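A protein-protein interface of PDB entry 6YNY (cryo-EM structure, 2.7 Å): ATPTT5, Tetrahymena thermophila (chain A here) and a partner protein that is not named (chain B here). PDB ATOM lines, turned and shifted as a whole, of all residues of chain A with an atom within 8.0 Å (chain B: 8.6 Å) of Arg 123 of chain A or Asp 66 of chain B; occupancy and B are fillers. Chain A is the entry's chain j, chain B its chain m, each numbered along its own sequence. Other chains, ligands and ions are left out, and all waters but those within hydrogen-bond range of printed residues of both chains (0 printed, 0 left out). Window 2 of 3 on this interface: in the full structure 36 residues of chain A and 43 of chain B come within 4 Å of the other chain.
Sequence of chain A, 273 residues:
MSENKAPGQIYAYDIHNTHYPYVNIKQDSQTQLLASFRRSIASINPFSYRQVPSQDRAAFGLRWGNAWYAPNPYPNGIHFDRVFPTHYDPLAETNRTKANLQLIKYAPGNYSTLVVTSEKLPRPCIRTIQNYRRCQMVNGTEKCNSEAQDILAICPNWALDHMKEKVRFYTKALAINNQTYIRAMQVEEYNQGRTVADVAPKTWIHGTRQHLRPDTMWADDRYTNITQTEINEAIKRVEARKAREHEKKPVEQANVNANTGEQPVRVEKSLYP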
ATOM      1  N   LYS A 120     -20.644  17.222 -16.544  1.00  0.00           N
ATOM      2  CA  LYS A 120     -19.761  18.279 -16.076  1.00  0.00           C
ATOM      3  C   LYS A 120     -19.581  18.151 -14.568  1.00  0.00           C
ATOM      4  O   LYS A 120     -20.554  18.242 -13.813  1.00  0.00           O
ATOM      5  CB  LYS A 120     -20.326  19.647 -16.443  1.00  0.00           C
ATOM      6  CG  LYS A 120     -19.425  20.794 -16.081  1.00  0.00           C
ATOM      7  CD  LYS A 120     -19.582  21.944 -17.051  1.00  0.00           C
ATOM      8  CE  LYS A 120     -20.991  22.494 -17.060  1.00  0.00           C
ATOM      9  NZ  LYS A 120     -21.138  23.563 -18.083  1.00  0.00           N
ATOM     10  N   LEU A 121     -18.340  17.935 -14.136  1.00  0.00           N
ATOM     11  CA  LEU A 121     -18.080  17.726 -12.726  1.00  0.00           C
ATOM     12  C   LEU A 121     -18.445  18.974 -11.928  1.00  0.00           C
ATOM     13  O   LEU A 121     -18.472  20.083 -12.466  1.00  0.00           O
ATOM     14  CB  LEU A 121     -16.615  17.369 -12.498  1.00  0.00           C
ATOM     15  CG  LEU A 121     -16.116  16.087 -13.163  1.00  0.00           C
ATOM     16  CD1 LEU A 121     -14.690  15.823 -12.776  1.00  0.00           C
ATOM     17  CD2 LEU A 121     -16.983  14.906 -12.801  1.00  0.00           C
ATOM     18  N   PRO A 122     -18.737  18.816 -10.638  1.00  0.00           N
ATOM     19  CA  PRO A 122     -19.122  19.972  -9.831  1.00  0.00           C
ATOM     20  C   PRO A 122     -18.037  21.034  -9.787  1.00  0.00           C
ATOM     21  O   PRO A 122     -16.842  20.744  -9.862  1.00  0.00           O
ATOM     22  CB  PRO A 122     -19.369  19.369  -8.445  1.00  0.00           C
ATOM     23  CG  PRO A 122     -19.653  17.956  -8.699  1.00  0.00           C
ATOM     24  CD  PRO A 122     -18.826  17.568  -9.866  1.00  0.00           C
ATOM     25  N   ARG A 123     -18.479  22.280  -9.660  1.00  0.00           N
ATOM     26  CA  ARG A 123     -17.548  23.399  -9.545  1.00  0.00           C
ATOM     27  C   ARG A 123     -16.560  23.220  -8.403  1.00  0.00           C
ATOM     28  O   ARG A 123     -15.350  23.388  -8.631  1.00  0.00           O
ATOM     29  CB  ARG A 123     -18.350  24.692  -9.395  1.00  0.00           C
ATOM     30  CG  ARG A 123     -17.529  25.953  -9.399  1.00  0.00           C
ATOM     31  CD  ARG A 123     -18.427  27.158  -9.532  1.00  0.00           C
ATOM     32  NE  ARG A 123     -19.033  27.230 -10.856  1.00  0.00           N
ATOM     33  CZ  ARG A 123     -20.126  27.926 -11.144  1.00  0.00           C
ATOM     34  NH1 ARG A 123     -20.750  28.613 -10.199  1.00  0.00           N
ATOM     35  NH2 ARG A 123     -20.600  27.930 -12.379  1.00  0.00           N
ATOM     36  N   PRO A 124     -16.977  22.893  -7.177  1.00  0.00           N
ATOM     37  CA  PRO A 124     -15.988  22.723  -6.105  1.00  0.00           C
ATOM     38  C   PRO A 124     -14.997  21.610  -6.372  1.00  0.00           C
ATOM     39  O   PRO A 124     -13.837  21.712  -5.957  1.00  0.00           O
ATOM     40  CB  PRO A 124     -16.853  22.428  -4.875  1.00  0.00           C
ATOM     41  CG  PRO A 124     -18.141  21.968  -5.407  1.00  0.00           C
ATOM     42  CD  PRO A 124     -18.348  22.679  -6.692  1.00  0.00           C
ATOM     43  N   CYS A 125     -15.419  20.545  -7.051  1.00  0.00           N
ATOM     44  CA  CYS A 125     -14.488  19.478  -7.392  1.00  0.00           C
ATOM     45  C   CYS A 125     -13.493  19.932  -8.447  1.00  0.00           C
ATOM     46  O   CYS A 125     -12.332  19.513  -8.426  1.00  0.00           O
ATOM     47  CB  CYS A 125     -15.253  18.247  -7.871  1.00  0.00           C
ATOM     48  SG  CYS A 125     -14.193  16.871  -8.326  1.00  0.00           S
ATOM     49  N   ILE A 126     -13.929  20.784  -9.375  1.00  0.00           N
ATOM     50  CA  ILE A 126     -13.026  21.313 -10.388  1.00  0.00           C
ATOM     51  C   ILE A 126     -11.964  22.190  -9.746  1.00  0.00           C
ATOM     52  O   ILE A 126     -10.791  22.158 -10.134  1.00  0.00           O
ATOM     53  CB  ILE A 126     -13.827  22.080 -11.454  1.00  0.00           C
ATOM     54  CG1 ILE A 126     -14.542  21.099 -12.377  1.00  0.00           C
ATOM     55  CG2 ILE A 126     -12.927  23.014 -12.230  1.00  0.00           C
ATOM     56  CD1 ILE A 126     -15.504  21.744 -13.335  1.00  0.00           C
ATOM     57  N   ARG A 127     -12.356  22.986  -8.753  1.00  0.00           N
ATOM     58  CA  ARG A 127     -11.412  23.883  -8.100  1.00  0.00           C
ATOM     59  C   ARG A 127     -10.327  23.119  -7.353  1.00  0.00           C
ATOM     60  O   ARG A 127      -9.183  23.579  -7.290  1.00  0.00           O
ATOM     61  CB  ARG A 127     -12.161  24.811  -7.151  1.00  0.00           C
ATOM     62  CG  ARG A 127     -13.152  25.724  -7.841  1.00  0.00           C
ATOM     63  CD  ARG A 127     -12.463  26.846  -8.592  1.00  0.00           C
ATOM     64  NE  ARG A 127     -13.245  27.303  -9.734  1.00  0.00           N
ATOM     65  CZ  ARG A 127     -14.199  28.224  -9.675  1.00  0.00           C
ATOM     66  NH1 ARG A 127     -14.506  28.804  -8.527  1.00  0.00           N
ATOM     67  NH2 ARG A 127     -14.853  28.565 -10.773  1.00  0.00           N
ATOM     68  N   THR A 128     -10.661  21.964  -6.777  1.00  0.00           N
ATOM     69  CA  THR A 128      -9.644  21.158  -6.114  1.00  0.00           C
ATOM     70  C   THR A 128      -8.637  20.609  -7.111  1.00  0.00           C
ATOM     71  O   THR A 128      -7.460  20.443  -6.777  1.00  0.00           O
ATOM     72  CB  THR A 128     -10.289  20.010  -5.342  1.00  0.00           C
ATOM     73  OG1 THR A 128     -11.085  19.216  -6.230  1.00  0.00           O
ATOM     74  CG2 THR A 128     -11.149  20.537  -4.226  1.00  0.00           C
ATOM     75  N   ILE A 129      -9.081  20.319  -8.332  1.00  0.00           N
ATOM     76  CA  ILE A 129      -8.172  19.825  -9.358  1.00  0.00           C
ATOM     77  C   ILE A 129      -7.274  20.949  -9.851  1.00  0.00           C
ATOM     78  O   ILE A 129      -6.087  20.741 -10.125  1.00  0.00           O
ATOM     79  CB  ILE A 129      -8.976  19.188 -10.504  1.00  0.00           C
ATOM     80  CG1 ILE A 129      -9.837  18.048  -9.967  1.00  0.00           C
ATOM     81  CG2 ILE A 129      -8.054  18.676 -11.583  1.00  0.00           C
ATOM     82  CD1 ILE A 129     -10.800  17.495 -10.960  1.00  0.00           C
ATOM     83  N   GLN A 130      -7.823  22.156  -9.977  1.00  0.00           N
ATOM     84  CA  GLN A 130      -7.014  23.293 -10.389  1.00  0.00           C
ATOM     85  C   GLN A 130      -5.951  23.622  -9.356  1.00  0.00           C
ATOM     86  O   GLN A 130      -4.849  24.054  -9.712  1.00  0.00           O
ATOM     87  CB  GLN A 130      -7.909  24.504 -10.630  1.00  0.00           C
ATOM     88  CG  GLN A 130      -8.857  24.333 -11.784  1.00  0.00           C
ATOM     89  CD  GLN A 130      -9.747  25.532 -11.994  1.00  0.00           C
ATOM     90  OE1 GLN A 130     -10.142  26.204 -11.044  1.00  0.00           O
ATOM     91  NE2 GLN A 130     -10.065  25.811 -13.247  1.00  0.00           N
ATOM     92  N   ILE A 154     -13.744  16.315  -1.080  1.00  0.00           N
ATOM     93  CA  ILE A 154     -14.761  17.249  -1.540  1.00  0.00           C
ATOM     94  C   ILE A 154     -15.482  16.721  -2.771  1.00  0.00           C
ATOM     95  O   ILE A 154     -16.702  16.854  -2.887  1.00  0.00           O
ATOM     96  CB  ILE A 154     -14.112  18.620  -1.800  1.00  0.00           C
ATOM     97  CG1 ILE A 154     -13.541  19.163  -0.493  1.00  0.00           C
ATOM     98  CG2 ILE A 154     -15.119  19.586  -2.388  1.00  0.00           C
ATOM     99  CD1 ILE A 154     -12.780  20.442  -0.627  1.00  0.00           C
ATOM    100  N   CYS A 155     -14.756  16.122  -3.697  1.00  0.00           N
ATOM    101  CA  CYS A 155     -15.376  15.596  -4.899  1.00  0.00           C
ATOM    102  C   CYS A 155     -16.312  14.456  -4.525  1.00  0.00           C
ATOM    103  O   CYS A 155     -15.873  13.504  -3.868  1.00  0.00           O
ATOM    104  CB  CYS A 155     -14.320  15.109  -5.886  1.00  0.00           C
ATOM    105  SG  CYS A 155     -13.274  16.391  -6.583  1.00  0.00           S
ATOM    106  N   PRO A 156     -17.588  14.501  -4.900  1.00  0.00           N
ATOM    107  CA  PRO A 156     -18.472  13.373  -4.602  1.00  0.00           C
ATOM    108  C   PRO A 156     -17.961  12.085  -5.225  1.00  0.00           C
ATOM    109  O   PRO A 156     -17.189  12.084  -6.185  1.00  0.00           O
ATOM    110  CB  PRO A 156     -19.815  13.802  -5.199  1.00  0.00           C
ATOM    111  CG  PRO A 156     -19.502  14.907  -6.121  1.00  0.00           C
ATOM    112  CD  PRO A 156     -18.315  15.589  -5.570  1.00  0.00           C
ATOM    113  N   PRO B  58     -14.177  28.100 -19.015  1.00  0.00           N
ATOM    114  CA  PRO B  58     -15.393  28.198 -18.197  1.00  0.00           C
ATOM    115  C   PRO B  58     -15.159  27.958 -16.718  1.00  0.00           C
ATOM    116  O   PRO B  58     -16.060  28.233 -15.918  1.00  0.00           O
ATOM    117  CB  PRO B  58     -16.301  27.120 -18.793  1.00  0.00           C
ATOM    118  CG  PRO B  58     -15.378  26.138 -19.374  1.00  0.00           C
ATOM    119  CD  PRO B  58     -14.192  26.899 -19.867  1.00  0.00           C
ATOM    120  N   THR B  59     -13.994  27.453 -16.330  1.00  0.00           N
ATOM    121  CA  THR B  59     -13.686  27.201 -14.932  1.00  0.00           C
ATOM    122  C   THR B  59     -13.079  28.410 -14.238  1.00  0.00           C
ATOM    123  O   THR B  59     -12.696  28.308 -13.068  1.00  0.00           O
ATOM    124  CB  THR B  59     -12.738  26.009 -14.808  1.00  0.00           C
ATOM    125  OG1 THR B  59     -11.460  26.346 -15.357  1.00  0.00           O
ATOM    126  CG2 THR B  59     -13.297  24.815 -15.552  1.00  0.00           C
ATOM    127  N   ASP B  60     -12.981  29.540 -14.923  1.00  0.00           N
ATOM    128  CA  ASP B  60     -12.486  30.749 -14.293  1.00  0.00           C
ATOM    129  C   ASP B  60     -13.481  31.226 -13.235  1.00  0.00           C
ATOM    130  O   ASP B  60     -14.691  31.221 -13.475  1.00  0.00           O
ATOM    131  CB  ASP B  60     -12.263  31.838 -15.340  1.00  0.00           C
ATOM    132  CG  ASP B  60     -11.610  33.079 -14.772  1.00  0.00           C
ATOM    133  OD1 ASP B  60     -12.059  33.569 -13.718  1.00  0.00           O
ATOM    134  OD2 ASP B  60     -10.643  33.570 -15.387  1.00  0.00           O
ATOM    135  N   PRO B  61     -13.007  31.638 -12.057  1.00  0.00           N
ATOM    136  CA  PRO B  61     -13.933  32.148 -11.036  1.00  0.00           C
ATOM    137  C   PRO B  61     -14.777  33.316 -11.499  1.00  0.00           C
ATOM    138  O   PRO B  61     -15.801  33.606 -10.869  1.00  0.00           O
ATOM    139  CB  PRO B  61     -12.996  32.559  -9.894  1.00  0.00           C
ATOM    140  CG  PRO B  61     -11.800  31.732 -10.080  1.00  0.00           C
ATOM    141  CD  PRO B  61     -11.633  31.543 -11.542  1.00  0.00           C
ATOM    142  N   GLU B  62     -14.388  33.999 -12.575  1.00  0.00           N
ATOM    143  CA  GLU B  62     -15.178  35.122 -13.062  1.00  0.00           C
ATOM    144  C   GLU B  62     -16.599  34.703 -13.402  1.00  0.00           C
ATOM    145  O   GLU B  62     -17.538  35.485 -13.214  1.00  0.00           O
ATOM    146  CB  GLU B  62     -14.503  35.735 -14.286  1.00  0.00           C
ATOM    147  CG  GLU B  62     -15.244  36.911 -14.875  1.00  0.00           C
ATOM    148  CD  GLU B  62     -14.547  37.491 -16.083  1.00  0.00           C
ATOM    149  OE1 GLU B  62     -13.504  36.941 -16.489  1.00  0.00           O
ATOM    150  OE2 GLU B  62     -15.041  38.501 -16.625  1.00  0.00           O
ATOM    151  N   TRP B  63     -16.780  33.483 -13.892  1.00  0.00           N
ATOM    152  CA  TRP B  63     -18.079  33.003 -14.335  1.00  0.00           C
ATOM    153  C   TRP B  63     -18.851  32.297 -13.231  1.00  0.00           C
ATOM    154  O   TRP B  63     -19.837  31.612 -13.519  1.00  0.00           O
ATOM    155  CB  TRP B  63     -17.902  32.071 -15.534  1.00  0.00           C
ATOM    156  CG  TRP B  63     -16.861  32.558 -16.483  1.00  0.00           C
ATOM    157  CD1 TRP B  63     -15.732  31.905 -16.861  1.00  0.00           C
ATOM    158  CD2 TRP B  63     -16.839  33.820 -17.158  1.00  0.00           C
ATOM    159  NE1 TRP B  63     -15.009  32.674 -17.734  1.00  0.00           N
ATOM    160  CE2 TRP B  63     -15.669  33.856 -17.934  1.00  0.00           C
ATOM    161  CE3 TRP B  63     -17.697  34.919 -17.185  1.00  0.00           C
ATOM    162  CZ2 TRP B  63     -15.337  34.944 -18.725  1.00  0.00           C
ATOM    163  CZ3 TRP B  63     -17.366  35.995 -17.971  1.00  0.00           C
ATOM    164  CH2 TRP B  63     -16.196  36.003 -18.730  1.00  0.00           C
ATOM    165  N   ASP B  64     -18.430  32.451 -11.979  1.00  0.00           N
ATOM    166  CA  ASP B  64     -19.166  31.918 -10.843  1.00  0.00           C
ATOM    167  C   ASP B  64     -20.376  32.764 -10.486  1.00  0.00           C
ATOM    168  O   ASP B  64     -21.087  32.432  -9.531  1.00  0.00           O
ATOM    169  CB  ASP B  64     -18.244  31.800  -9.630  1.00  0.00           C
ATOM    170  CG  ASP B  64     -17.230  30.688  -9.773  1.00  0.00           C
ATOM    171  OD1 ASP B  64     -17.176  30.063 -10.851  1.00  0.00           O
ATOM    172  OD2 ASP B  64     -16.490  30.432  -8.802  1.00  0.00           O
ATOM    173  N   ASP B  65     -20.625  33.845 -11.223  1.00  0.00           N
ATOM    174  CA  ASP B  65     -21.771  34.695 -10.932  1.00  0.00           C
ATOM    175  C   ASP B  65     -23.086  33.980 -11.204  1.00  0.00           C
ATOM    176  O   ASP B  65     -24.109  34.319 -10.598  1.00  0.00           O
ATOM    177  CB  ASP B  65     -21.683  35.981 -11.750  1.00  0.00           C
ATOM    178  CG  ASP B  65     -21.593  35.726 -13.243  1.00  0.00           C
ATOM    179  OD1 ASP B  65     -22.557  35.182 -13.819  1.00  0.00           O
ATOM    180  OD2 ASP B  65     -20.559  36.081 -13.844  1.00  0.00           O
ATOM    181  N   ASP B  66     -23.084  32.997 -12.101  1.00  0.00           N
ATOM    182  CA  ASP B  66     -24.294  32.259 -12.451  1.00  0.00           C
ATOM    183  C   ASP B  66     -25.414  33.214 -12.848  1.00  0.00           C
ATOM    184  O   ASP B  66     -26.566  33.069 -12.438  1.00  0.00           O
ATOM    185  CB  ASP B  66     -24.729  31.350 -11.303  1.00  0.00           C
ATOM    186  CG  ASP B  66     -23.762  30.207 -11.067  1.00  0.00           C
ATOM    187  OD1 ASP B  66     -22.729  30.147 -11.765  1.00  0.00           O
ATOM    188  OD2 ASP B  66     -24.036  29.364 -10.189  1.00  0.00           O
ATOM    189  N   MET B  67     -25.063  34.207 -13.656  1.00  0.00           N
ATOM    190  CA  MET B  67     -26.018  35.221 -14.063  1.00  0.00           C
ATOM    191  C   MET B  67     -27.027  34.657 -15.054  1.00  0.00           C
ATOM    192  O   MET B  67     -26.728  33.753 -15.839  1.00  0.00           O
ATOM    193  CB  MET B  67     -25.287  36.405 -14.681  1.00  0.00           C
ATOM    194  CG  MET B  67     -26.185  37.540 -15.100  1.00  0.00           C
ATOM    195  SD  MET B  67     -27.233  38.147 -13.774  1.00  0.00           S
ATOM    196  CE  MET B  67     -28.140  39.403 -14.654  1.00  0.00           C
ATOM    197  N   THR B  68     -28.236  35.206 -15.009  1.00  0.00           N
ATOM    198  CA  THR B  68     -29.324  34.807 -15.880  1.00  0.00           C
ATOM    199  C   THR B  68     -29.437  35.771 -17.057  1.00  0.00           C
ATOM    200  O   THR B  68     -28.723  36.771 -17.153  1.00  0.00           O
ATOM    201  CB  THR B  68     -30.643  34.764 -15.105  1.00  0.00           C
ATOM    202  OG1 THR B  68     -30.924  36.058 -14.564  1.00  0.00           O
ATOM    203  CG2 THR B  68     -30.570  33.772 -13.986  1.00  0.00           C
ATOM    204  N   TYR B  69     -30.360  35.459 -17.962  1.00  0.00           N
ATOM    205  CA  TYR B  69     -30.655  36.317 -19.097  1.00  0.00           C
ATOM    206  C   TYR B  69     -31.840  37.208 -18.766  1.00  0.00           C
ATOM    207  O   TYR B  69     -32.956  36.693 -18.597  1.00  0.00           O
ATOM    208  CB  TYR B  69     -30.961  35.483 -20.336  1.00  0.00           C
ATOM    209  CG  TYR B  69     -29.774  34.850 -21.008  1.00  0.00           C
ATOM    210  CD1 TYR B  69     -29.039  35.546 -21.949  1.00  0.00           C
ATOM    211  CD2 TYR B  69     -29.406  33.547 -20.730  1.00  0.00           C
ATOM    212  CE1 TYR B  69     -27.971  34.972 -22.578  1.00  0.00           C
ATOM    213  CE2 TYR B  69     -28.337  32.964 -21.354  1.00  0.00           C
ATOM    214  CZ  TYR B  69     -27.621  33.680 -22.278  1.00  0.00           C
ATOM    215  OH  TYR B  69     -26.550  33.097 -22.906  1.00  0.00           O
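NE of Arg 123 of chain A is in salt-bridge range of OD1 of Asp 64 of chain B, 3.4 Å away. The guanidinium group of Arg 123 of chain A lies within salt-bridge range of the side-chain carboxylate of Asp 66 of chain B, 3.0 Å away. NH2 of Arg 127 of chain A lies within hydrogen-bond range of O of Thr 59 of chain B, 3.2 Å away. NH1 of Arg 127 of chain A lies within salt-bridge range of OD2 of Asp 64 of chain B, at 2.6 Å. The side-chain amide nitrogen (NE2) of Gln 130 of chain A sits at hydrogen-bond distance from the side-chain hydroxyl (OG1) of Thr 59 of chain B (2.6 Å).
Arg 123 of chain A touches Trp 63 of chain B. CG2 of Ile 126 of chain A touches CG2 of Thr 59 of chain B (3.8 Å). Asp 60 of chain B touches Arg 127 of chain A (O to NH2, 3.8 Å). NH2 of Arg 127 of chain A touches CA of Pro 61 of chain B, at 3.7 Å.
Asp 66 of chain B touches just one residue of chain A: Arg 123 (3.0 Å). Of the printed residues of chain A, Asp 60 of chain B touches Arg 127 (3.8 Å). Of the printed residues of chain B, Gln 130 of chain A touches Thr 59 (2.6 Å). Printed residues of chain A within 4 Å of Thr 59 of chain B: Ile 126 (3.8 Å), Arg 127 (3.2 Å) and Gln 130 (2.6 Å). Of the printed residues of chain B, Ile 126 of chain A touches Thr 59 (3.8 Å). Glu 62 of chain B touches none of the printed residues of chain A. The nearest printed residue of chain A that does not touch Asp 66 of chain B is Arg 127 of chain A (8.1 Å).
The side-chain carboxylate (OD1) of Asp 60 of chain B lies within hydrogen-bond range of the backbone NH (N) of Glu 62 of chain B. The side-chain sulfur (SG) of Cys 125 of chain A is disulfide-bonded to the side-chain sulfur (SG) of Cys 155 of chain A (2.0 Å).
Of the 14 printed residues of chain A, 4 touch a printed residue of chain B. Among the printed residues, Asp or Glu carboxylates within 4 Å of a Lys or Arg side-chain nitrogen of the other chain: Arg 123 of chain A with Asp 64 of chain B, Arg 123 of chain A with Asp 66 of chain B and Arg 127 of chain A with Asp 64 of chain B.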
